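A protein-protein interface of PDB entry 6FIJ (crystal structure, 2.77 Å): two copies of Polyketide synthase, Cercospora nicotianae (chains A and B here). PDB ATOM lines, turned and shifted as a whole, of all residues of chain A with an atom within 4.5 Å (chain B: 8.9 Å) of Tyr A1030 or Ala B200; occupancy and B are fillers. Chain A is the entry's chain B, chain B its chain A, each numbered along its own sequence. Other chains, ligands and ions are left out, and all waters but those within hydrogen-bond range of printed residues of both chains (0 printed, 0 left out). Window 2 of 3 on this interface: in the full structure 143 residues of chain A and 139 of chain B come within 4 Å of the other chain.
OH of Tyr A1030 sits at hydrogen-bond distance from O of Ala B200 (3.4 Å). The backbone carbonyl oxygen of Leu B162 lies within hydrogen-bond range of the side-chain hydroxyl of Ser A1026 (3.1 Å).
O of Asp A1027 lies within hydrogen-bond range of SG of Cys A1134.
Among the printed residues, merely in contact across the chains: Met A958 with Ser B203 (3.4 Å), Met A958 with Val B204 (3.7 Å), Asp A1027 with Ser B205 (3.6 Å), Tyr A1030 with Ala B202 (3.4 Å), Gln A1129 with Ala B200 (3.9 Å), Ala A1133 with Gln B199 (3.9 Å), Ala A1133 with Ala B200 (3.2 Å) and Ala A1133 with Leu B201 (3.9 Å).
Of the printed residues of chain B, Met A958 touches Ser B203 (3.4 Å) and Val B204 (3.7 Å). Of the printed residues of chain B, Ser A1026 touches Leu B162 (3.1 Å). Of the printed residues of chain B, Gln A1129 touches Ala B200 (3.9 Å). Of the printed residues of chain A, Gln B199 touches Ala A1133. The nearest printed residue of chain A that does not touch Ala B200 is Val A1130 (5.7 Å). The nearest printed residue of chain B that does not touch Asp A1027 is Leu B162 (4.7 Å).
Of the 14 printed residues of chain A, 6 touch a printed residue of chain B. Among the printed residues, no Asp or Glu carboxylate lies within 4 Å of a Lys or Arg side-chain nitrogen of the other chain.
No position is printed for both chains. Of the 10 pairs that touch across the chains among the printed residues, none has its exchanged pair printed and touching as well.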
ATOM      1  N   MET A 958       0.701  -2.745 -32.010  1.00  0.00           N
ATOM      2  CA  MET A 958      -0.679  -3.024 -31.639  1.00  0.00           C
ATOM      3  C   MET A 958      -1.596  -3.144 -32.851  1.00  0.00           C
ATOM      4  O   MET A 958      -2.816  -3.005 -32.713  1.00  0.00           O
ATOM      5  CB  MET A 958      -1.200  -1.927 -30.711  1.00  0.00           C
ATOM      6  CG  MET A 958      -0.406  -1.780 -29.435  1.00  0.00           C
ATOM      7  SD  MET A 958      -1.161  -0.606 -28.299  1.00  0.00           S
ATOM      8  CE  MET A 958      -1.047   0.907 -29.238  1.00  0.00           C
ATOM      9  N   SER A1026       1.496   4.541 -24.266  1.00  0.00           N
ATOM     10  CA  SER A1026       1.038   3.413 -25.071  1.00  0.00           C
ATOM     11  C   SER A1026      -0.422   3.081 -24.789  1.00  0.00           C
ATOM     12  O   SER A1026      -1.183   2.775 -25.713  1.00  0.00           O
ATOM     13  CB  SER A1026       1.920   2.191 -24.820  1.00  0.00           C
ATOM     14  OG  SER A1026       1.754   1.706 -23.500  1.00  0.00           O
ATOM     15  N   ASP A1027      -0.834   3.126 -23.519  1.00  0.00           N
ATOM     16  CA  ASP A1027      -2.235   2.878 -23.199  1.00  0.00           C
ATOM     17  C   ASP A1027      -3.137   3.931 -23.826  1.00  0.00           C
ATOM     18  O   ASP A1027      -4.261   3.622 -24.237  1.00  0.00           O
ATOM     19  CB  ASP A1027      -2.437   2.837 -21.683  1.00  0.00           C
ATOM     20  CG  ASP A1027      -1.916   1.553 -21.058  1.00  0.00           C
ATOM     21  OD1 ASP A1027      -1.677   0.578 -21.803  1.00  0.00           O
ATOM     22  OD2 ASP A1027      -1.753   1.517 -19.819  1.00  0.00           O
ATOM     23  N   THR A1028      -2.664   5.175 -23.910  1.00  0.00           N
ATOM     24  CA  THR A1028      -3.423   6.214 -24.596  1.00  0.00           C
ATOM     25  C   THR A1028      -3.614   5.866 -26.067  1.00  0.00           C
ATOM     26  O   THR A1028      -4.732   5.928 -26.593  1.00  0.00           O
ATOM     27  CB  THR A1028      -2.712   7.560 -24.444  1.00  0.00           C
ATOM     28  OG1 THR A1028      -2.714   7.943 -23.062  1.00  0.00           O
ATOM     29  CG2 THR A1028      -3.400   8.645 -25.267  1.00  0.00           C
ATOM     30  N   LEU A1029      -2.526   5.502 -26.751  1.00  0.00           N
ATOM     31  CA  LEU A1029      -2.619   5.142 -28.162  1.00  0.00           C
ATOM     32  C   LEU A1029      -3.509   3.924 -28.368  1.00  0.00           C
ATOM     33  O   LEU A1029      -4.310   3.883 -29.308  1.00  0.00           O
ATOM     34  CB  LEU A1029      -1.221   4.879 -28.724  1.00  0.00           C
ATOM     35  CG  LEU A1029      -0.234   6.043 -28.664  1.00  0.00           C
ATOM     36  CD1 LEU A1029       1.155   5.584 -29.078  1.00  0.00           C
ATOM     37  CD2 LEU A1029      -0.705   7.182 -29.549  1.00  0.00           C
ATOM     38  N   TYR A1030      -3.369   2.912 -27.509  1.00  0.00           N
ATOM     39  CA  TYR A1030      -4.232   1.738 -27.593  1.00  0.00           C
ATOM     40  C   TYR A1030      -5.694   2.131 -27.445  1.00  0.00           C
ATOM     41  O   TYR A1030      -6.551   1.709 -28.231  1.00  0.00           O
ATOM     42  CB  TYR A1030      -3.833   0.729 -26.513  1.00  0.00           C
ATOM     43  CG  TYR A1030      -4.701  -0.510 -26.447  1.00  0.00           C
ATOM     44  CD1 TYR A1030      -4.695  -1.441 -27.477  1.00  0.00           C
ATOM     45  CD2 TYR A1030      -5.501  -0.762 -25.342  1.00  0.00           C
ATOM     46  CE1 TYR A1030      -5.478  -2.582 -27.417  1.00  0.00           C
ATOM     47  CE2 TYR A1030      -6.284  -1.901 -25.272  1.00  0.00           C
ATOM     48  CZ  TYR A1030      -6.269  -2.807 -26.312  1.00  0.00           C
ATOM     49  OH  TYR A1030      -7.047  -3.940 -26.248  1.00  0.00           O
ATOM     50  N   LEU A1031      -5.994   2.955 -26.442  1.00  0.00           N
ATOM     51  CA  LEU A1031      -7.376   3.336 -26.175  1.00  0.00           C
ATOM     52  C   LEU A1031      -7.951   4.172 -27.312  1.00  0.00           C
ATOM     53  O   LEU A1031      -9.102   3.972 -27.715  1.00  0.00           O
ATOM     54  CB  LEU A1031      -7.441   4.094 -24.850  1.00  0.00           C
ATOM     55  CG  LEU A1031      -8.802   4.349 -24.204  1.00  0.00           C
ATOM     56  CD1 LEU A1031      -9.653   3.087 -24.123  1.00  0.00           C
ATOM     57  CD2 LEU A1031      -8.572   4.923 -22.819  1.00  0.00           C
ATOM     58  N   VAL A1032      -7.169   5.112 -27.845  1.00  0.00           N
ATOM     59  CA  VAL A1032      -7.652   5.948 -28.939  1.00  0.00           C
ATOM     60  C   VAL A1032      -7.780   5.128 -30.216  1.00  0.00           C
ATOM     61  O   VAL A1032      -8.796   5.192 -30.917  1.00  0.00           O
ATOM     62  CB  VAL A1032      -6.726   7.161 -29.138  1.00  0.00           C
ATOM     63  CG1 VAL A1032      -7.116   7.941 -30.397  1.00  0.00           C
ATOM     64  CG2 VAL A1032      -6.767   8.061 -27.914  1.00  0.00           C
ATOM     65  N   GLY A1033      -6.744   4.354 -30.544  1.00  0.00           N
ATOM     66  CA  GLY A1033      -6.775   3.576 -31.771  1.00  0.00           C
ATOM     67  C   GLY A1033      -7.917   2.580 -31.792  1.00  0.00           C
ATOM     68  O   GLY A1033      -8.684   2.514 -32.755  1.00  0.00           O
ATOM     69  N   ARG A1034      -8.043   1.787 -30.726  1.00  0.00           N
ATOM     70  CA  ARG A1034      -9.149   0.842 -30.640  1.00  0.00           C
ATOM     71  C   ARG A1034     -10.489   1.560 -30.749  1.00  0.00           C
ATOM     72  O   ARG A1034     -11.398   1.091 -31.443  1.00  0.00           O
ATOM     73  CB  ARG A1034      -9.069   0.052 -29.334  1.00  0.00           C
ATOM     74  CG  ARG A1034      -7.863  -0.872 -29.234  1.00  0.00           C
ATOM     75  CD  ARG A1034      -7.997  -2.103 -30.118  1.00  0.00           C
ATOM     76  NE  ARG A1034      -9.091  -2.976 -29.689  1.00  0.00           N
ATOM     77  CZ  ARG A1034     -10.286  -3.054 -30.274  1.00  0.00           C
ATOM     78  NH1 ARG A1034     -10.573  -2.318 -31.341  1.00  0.00           N
ATOM     79  NH2 ARG A1034     -11.203  -3.883 -29.790  1.00  0.00           N
ATOM     80  N   GLN A1129     -14.377  -2.529 -22.398  1.00  0.00           N
ATOM     81  CA  GLN A1129     -13.367  -3.562 -22.205  1.00  0.00           C
ATOM     82  C   GLN A1129     -11.974  -3.061 -22.566  1.00  0.00           C
ATOM     83  O   GLN A1129     -10.987  -3.487 -21.956  1.00  0.00           O
ATOM     84  CB  GLN A1129     -13.722  -4.796 -23.035  1.00  0.00           C
ATOM     85  CG  GLN A1129     -14.604  -5.790 -22.300  1.00  0.00           C
ATOM     86  CD  GLN A1129     -13.886  -6.462 -21.147  1.00  0.00           C
ATOM     87  OE1 GLN A1129     -14.266  -6.304 -19.986  1.00  0.00           O
ATOM     88  NE2 GLN A1129     -12.839  -7.217 -21.462  1.00  0.00           N
ATOM     89  N   VAL A1130     -11.873  -2.170 -23.553  1.00  0.00           N
ATOM     90  CA  VAL A1130     -10.577  -1.608 -23.917  1.00  0.00           C
ATOM     91  C   VAL A1130     -10.022  -0.773 -22.770  1.00  0.00           C
ATOM     92  O   VAL A1130      -8.819  -0.808 -22.483  1.00  0.00           O
ATOM     93  CB  VAL A1130     -10.700  -0.785 -25.213  1.00  0.00           C
ATOM     94  CG1 VAL A1130      -9.370  -0.142 -25.572  1.00  0.00           C
ATOM     95  CG2 VAL A1130     -11.174  -1.666 -26.355  1.00  0.00           C
ATOM     96  N   ALA A1133      -8.454  -2.643 -19.879  1.00  0.00           N
ATOM     97  CA  ALA A1133      -7.120  -3.172 -20.126  1.00  0.00           C
ATOM     98  C   ALA A1133      -6.023  -2.178 -19.772  1.00  0.00           C
ATOM     99  O   ALA A1133      -4.876  -2.590 -19.569  1.00  0.00           O
ATOM    100  CB  ALA A1133      -6.985  -3.585 -21.593  1.00  0.00           C
ATOM    101  N   CYS A1134      -6.343  -0.889 -19.706  1.00  0.00           N
ATOM    102  CA  CYS A1134      -5.351   0.135 -19.417  1.00  0.00           C
ATOM    103  C   CYS A1134      -5.102   0.244 -17.915  1.00  0.00           C
ATOM    104  O   CYS A1134      -5.966  -0.076 -17.094  1.00  0.00           O
ATOM    105  CB  CYS A1134      -5.800   1.487 -19.971  1.00  0.00           C
ATOM    106  SG  CYS A1134      -6.120   1.483 -21.750  1.00  0.00           S
ATOM    107  N   LEU B 162       5.758   2.712 -22.247  1.00  0.00           N
ATOM    108  CA  LEU B 162       4.793   1.649 -22.000  1.00  0.00           C
ATOM    109  C   LEU B 162       4.061   1.859 -20.677  1.00  0.00           C
ATOM    110  O   LEU B 162       2.826   1.869 -20.638  1.00  0.00           O
ATOM    111  CB  LEU B 162       5.509   0.296 -22.020  1.00  0.00           C
ATOM    112  CG  LEU B 162       4.666  -0.973 -21.889  1.00  0.00           C
ATOM    113  CD1 LEU B 162       3.608  -1.050 -22.980  1.00  0.00           C
ATOM    114  CD2 LEU B 162       5.566  -2.197 -21.929  1.00  0.00           C
ATOM    115  N   SER B 193      -0.657 -16.864 -21.925  1.00  0.00           N
ATOM    116  CA  SER B 193      -1.644 -16.661 -22.981  1.00  0.00           C
ATOM    117  C   SER B 193      -3.053 -16.591 -22.408  1.00  0.00           C
ATOM    118  O   SER B 193      -3.861 -15.753 -22.826  1.00  0.00           O
ATOM    119  CB  SER B 193      -1.546 -17.786 -24.013  1.00  0.00           C
ATOM    120  OG  SER B 193      -0.262 -17.828 -24.610  1.00  0.00           O
ATOM    121  N   ALA B 194      -3.367 -17.463 -21.449  1.00  0.00           N
ATOM    122  CA  ALA B 194      -4.692 -17.454 -20.840  1.00  0.00           C
ATOM    123  C   ALA B 194      -4.936 -16.162 -20.068  1.00  0.00           C
ATOM    124  O   ALA B 194      -5.964 -15.502 -20.253  1.00  0.00           O
ATOM    125  CB  ALA B 194      -4.851 -18.666 -19.922  1.00  0.00           C
ATOM    126  N   TYR B 195      -3.999 -15.786 -19.196  1.00  0.00           N
ATOM    127  CA  TYR B 195      -4.126 -14.529 -18.464  1.00  0.00           C
ATOM    128  C   TYR B 195      -4.309 -13.357 -19.420  1.00  0.00           C
ATOM    129  O   TYR B 195      -5.119 -12.457 -19.167  1.00  0.00           O
ATOM    130  CB  TYR B 195      -2.898 -14.315 -17.577  1.00  0.00           C
ATOM    131  CG  TYR B 195      -2.955 -13.059 -16.739  1.00  0.00           C
ATOM    132  CD1 TYR B 195      -3.674 -13.025 -15.551  1.00  0.00           C
ATOM    133  CD2 TYR B 195      -2.283 -11.909 -17.130  1.00  0.00           C
ATOM    134  CE1 TYR B 195      -3.727 -11.878 -14.780  1.00  0.00           C
ATOM    135  CE2 TYR B 195      -2.330 -10.759 -16.366  1.00  0.00           C
ATOM    136  CZ  TYR B 195      -3.053 -10.749 -15.194  1.00  0.00           C
ATOM    137  OH  TYR B 195      -3.099  -9.604 -14.432  1.00  0.00           O
ATOM    138  N   THR B 196      -3.563 -13.354 -20.526  1.00  0.00           N
ATOM    139  CA  THR B 196      -3.698 -12.297 -21.523  1.00  0.00           C
ATOM    140  C   THR B 196      -5.126 -12.219 -22.052  1.00  0.00           C
ATOM    141  O   THR B 196      -5.721 -11.138 -22.115  1.00  0.00           O
ATOM    142  CB  THR B 196      -2.721 -12.544 -22.673  1.00  0.00           C
ATOM    143  OG1 THR B 196      -1.381 -12.554 -22.169  1.00  0.00           O
ATOM    144  CG2 THR B 196      -2.855 -11.460 -23.739  1.00  0.00           C
ATOM    145  N   ALA B 197      -5.690 -13.366 -22.441  1.00  0.00           N
ATOM    146  CA  ALA B 197      -7.025 -13.380 -23.028  1.00  0.00           C
ATOM    147  C   ALA B 197      -8.058 -12.795 -22.075  1.00  0.00           C
ATOM    148  O   ALA B 197      -8.929 -12.023 -22.490  1.00  0.00           O
ATOM    149  CB  ALA B 197      -7.408 -14.805 -23.420  1.00  0.00           C
ATOM    150  N   GLU B 198      -7.974 -13.146 -20.790  1.00  0.00           N
ATOM    151  CA  GLU B 198      -9.020 -12.762 -19.848  1.00  0.00           C
ATOM    152  C   GLU B 198      -8.989 -11.271 -19.541  1.00  0.00           C
ATOM    153  O   GLU B 198     -10.038 -10.674 -19.276  1.00  0.00           O
ATOM    154  CB  GLU B 198      -8.875 -13.563 -18.554  1.00  0.00           C
ATOM    155  CG  GLU B 198      -9.044 -15.065 -18.729  1.00  0.00           C
ATOM    156  CD  GLU B 198      -8.491 -15.856 -17.558  1.00  0.00           C
ATOM    157  OE1 GLU B 198      -7.772 -15.265 -16.723  1.00  0.00           O
ATOM    158  OE2 GLU B 198      -8.775 -17.069 -17.474  1.00  0.00           O
ATOM    159  N   GLN B 199      -7.810 -10.652 -19.571  1.00  0.00           N
ATOM    160  CA  GLN B 199      -7.682  -9.236 -19.264  1.00  0.00           C
ATOM    161  C   GLN B 199      -7.800  -8.341 -20.493  1.00  0.00           C
ATOM    162  O   GLN B 199      -7.894  -7.119 -20.338  1.00  0.00           O
ATOM    163  CB  GLN B 199      -6.340  -8.968 -18.574  1.00  0.00           C
ATOM    164  CG  GLN B 199      -6.124  -9.762 -17.295  1.00  0.00           C
ATOM    165  CD  GLN B 199      -7.156  -9.452 -16.229  1.00  0.00           C
ATOM    166  OE1 GLN B 199      -7.708  -8.353 -16.181  1.00  0.00           O
ATOM    167  NE2 GLN B 199      -7.422 -10.424 -15.363  1.00  0.00           N
ATOM    168  N   ALA B 200      -7.797  -8.913 -21.700  1.00  0.00           N
ATOM    169  CA  ALA B 200      -7.894  -8.136 -22.935  1.00  0.00           C
ATOM    170  C   ALA B 200      -6.730  -7.158 -23.078  1.00  0.00           C
ATOM    171  O   ALA B 200      -6.885  -6.065 -23.629  1.00  0.00           O
ATOM    172  CB  ALA B 200      -9.228  -7.388 -23.013  1.00  0.00           C
ATOM    173  N   LEU B 201      -5.556  -7.550 -22.586  1.00  0.00           N
ATOM    174  CA  LEU B 201      -4.389  -6.677 -22.624  1.00  0.00           C
ATOM    175  C   LEU B 201      -3.985  -6.353 -24.056  1.00  0.00           C
ATOM    176  O   LEU B 201      -4.097  -7.186 -24.959  1.00  0.00           O
ATOM    177  CB  LEU B 201      -3.215  -7.329 -21.892  1.00  0.00           C
ATOM    178  CG  LEU B 201      -3.347  -7.444 -20.372  1.00  0.00           C
ATOM    179  CD1 LEU B 201      -2.301  -8.391 -19.812  1.00  0.00           C
ATOM    180  CD2 LEU B 201      -3.218  -6.072 -19.732  1.00  0.00           C
ATOM    181  N   ALA B 202      -3.509  -5.126 -24.254  1.00  0.00           N
ATOM    182  CA  ALA B 202      -2.900  -4.755 -25.522  1.00  0.00           C
ATOM    183  C   ALA B 202      -1.630  -5.565 -25.749  1.00  0.00           C
ATOM    184  O   ALA B 202      -0.918  -5.923 -24.807  1.00  0.00           O
ATOM    185  CB  ALA B 202      -2.579  -3.261 -25.540  1.00  0.00           C
ATOM    186  N   SER B 203      -1.351  -5.854 -27.023  1.00  0.00           N
ATOM    187  CA  SER B 203      -0.225  -6.718 -27.364  1.00  0.00           C
ATOM    188  C   SER B 203       1.080  -6.235 -26.748  1.00  0.00           C
ATOM    189  O   SER B 203       1.939  -7.052 -26.401  1.00  0.00           O
ATOM    190  CB  SER B 203      -0.081  -6.810 -28.884  1.00  0.00           C
ATOM    191  OG  SER B 203       0.055  -5.522 -29.459  1.00  0.00           O
ATOM    192  N   VAL B 204       1.257  -4.918 -26.615  1.00  0.00           N
ATOM    193  CA  VAL B 204       2.518  -4.395 -26.096  1.00  0.00           C
ATOM    194  C   VAL B 204       2.617  -4.557 -24.582  1.00  0.00           C
ATOM    195  O   VAL B 204       3.715  -4.756 -24.049  1.00  0.00           O
ATOM    196  CB  VAL B 204       2.696  -2.918 -26.494  1.00  0.00           C
ATOM    197  CG1 VAL B 204       2.839  -2.785 -28.001  1.00  0.00           C
ATOM    198  CG2 VAL B 204       1.535  -2.067 -25.977  1.00  0.00           C
ATOM    199  N   SER B 205       1.500  -4.469 -23.865  1.00  0.00           N
ATOM    200  CA  SER B 205       1.511  -4.508 -22.410  1.00  0.00           C
ATOM    201  C   SER B 205       1.445  -5.919 -21.844  1.00  0.00           C
ATOM    202  O   SER B 205       1.394  -6.078 -20.622  1.00  0.00           O
ATOM    203  CB  SER B 205       0.343  -3.685 -21.856  1.00  0.00           C
ATOM    204  OG  SER B 205       0.406  -2.341 -22.304  1.00  0.00           O
ATOM    205  N   VAL B 206       1.449  -6.941 -22.692  1.00  0.00           N
ATOM    206  CA  VAL B 206       1.267  -8.316 -22.236  1.00  0.00           C
ATOM    207  C   VAL B 206       2.509  -8.755 -21.468  1.00  0.00           C
ATOM    208  O   VAL B 206       3.616  -8.294 -21.779  1.00  0.00           O
ATOM    209  CB  VAL B 206       0.988  -9.252 -23.425  1.00  0.00           C
ATOM    210  CG1 VAL B 206       2.240  -9.432 -24.286  1.00  0.00           C
ATOM    211  CG2 VAL B 206       0.465 -10.586 -22.942  1.00  0.00           C
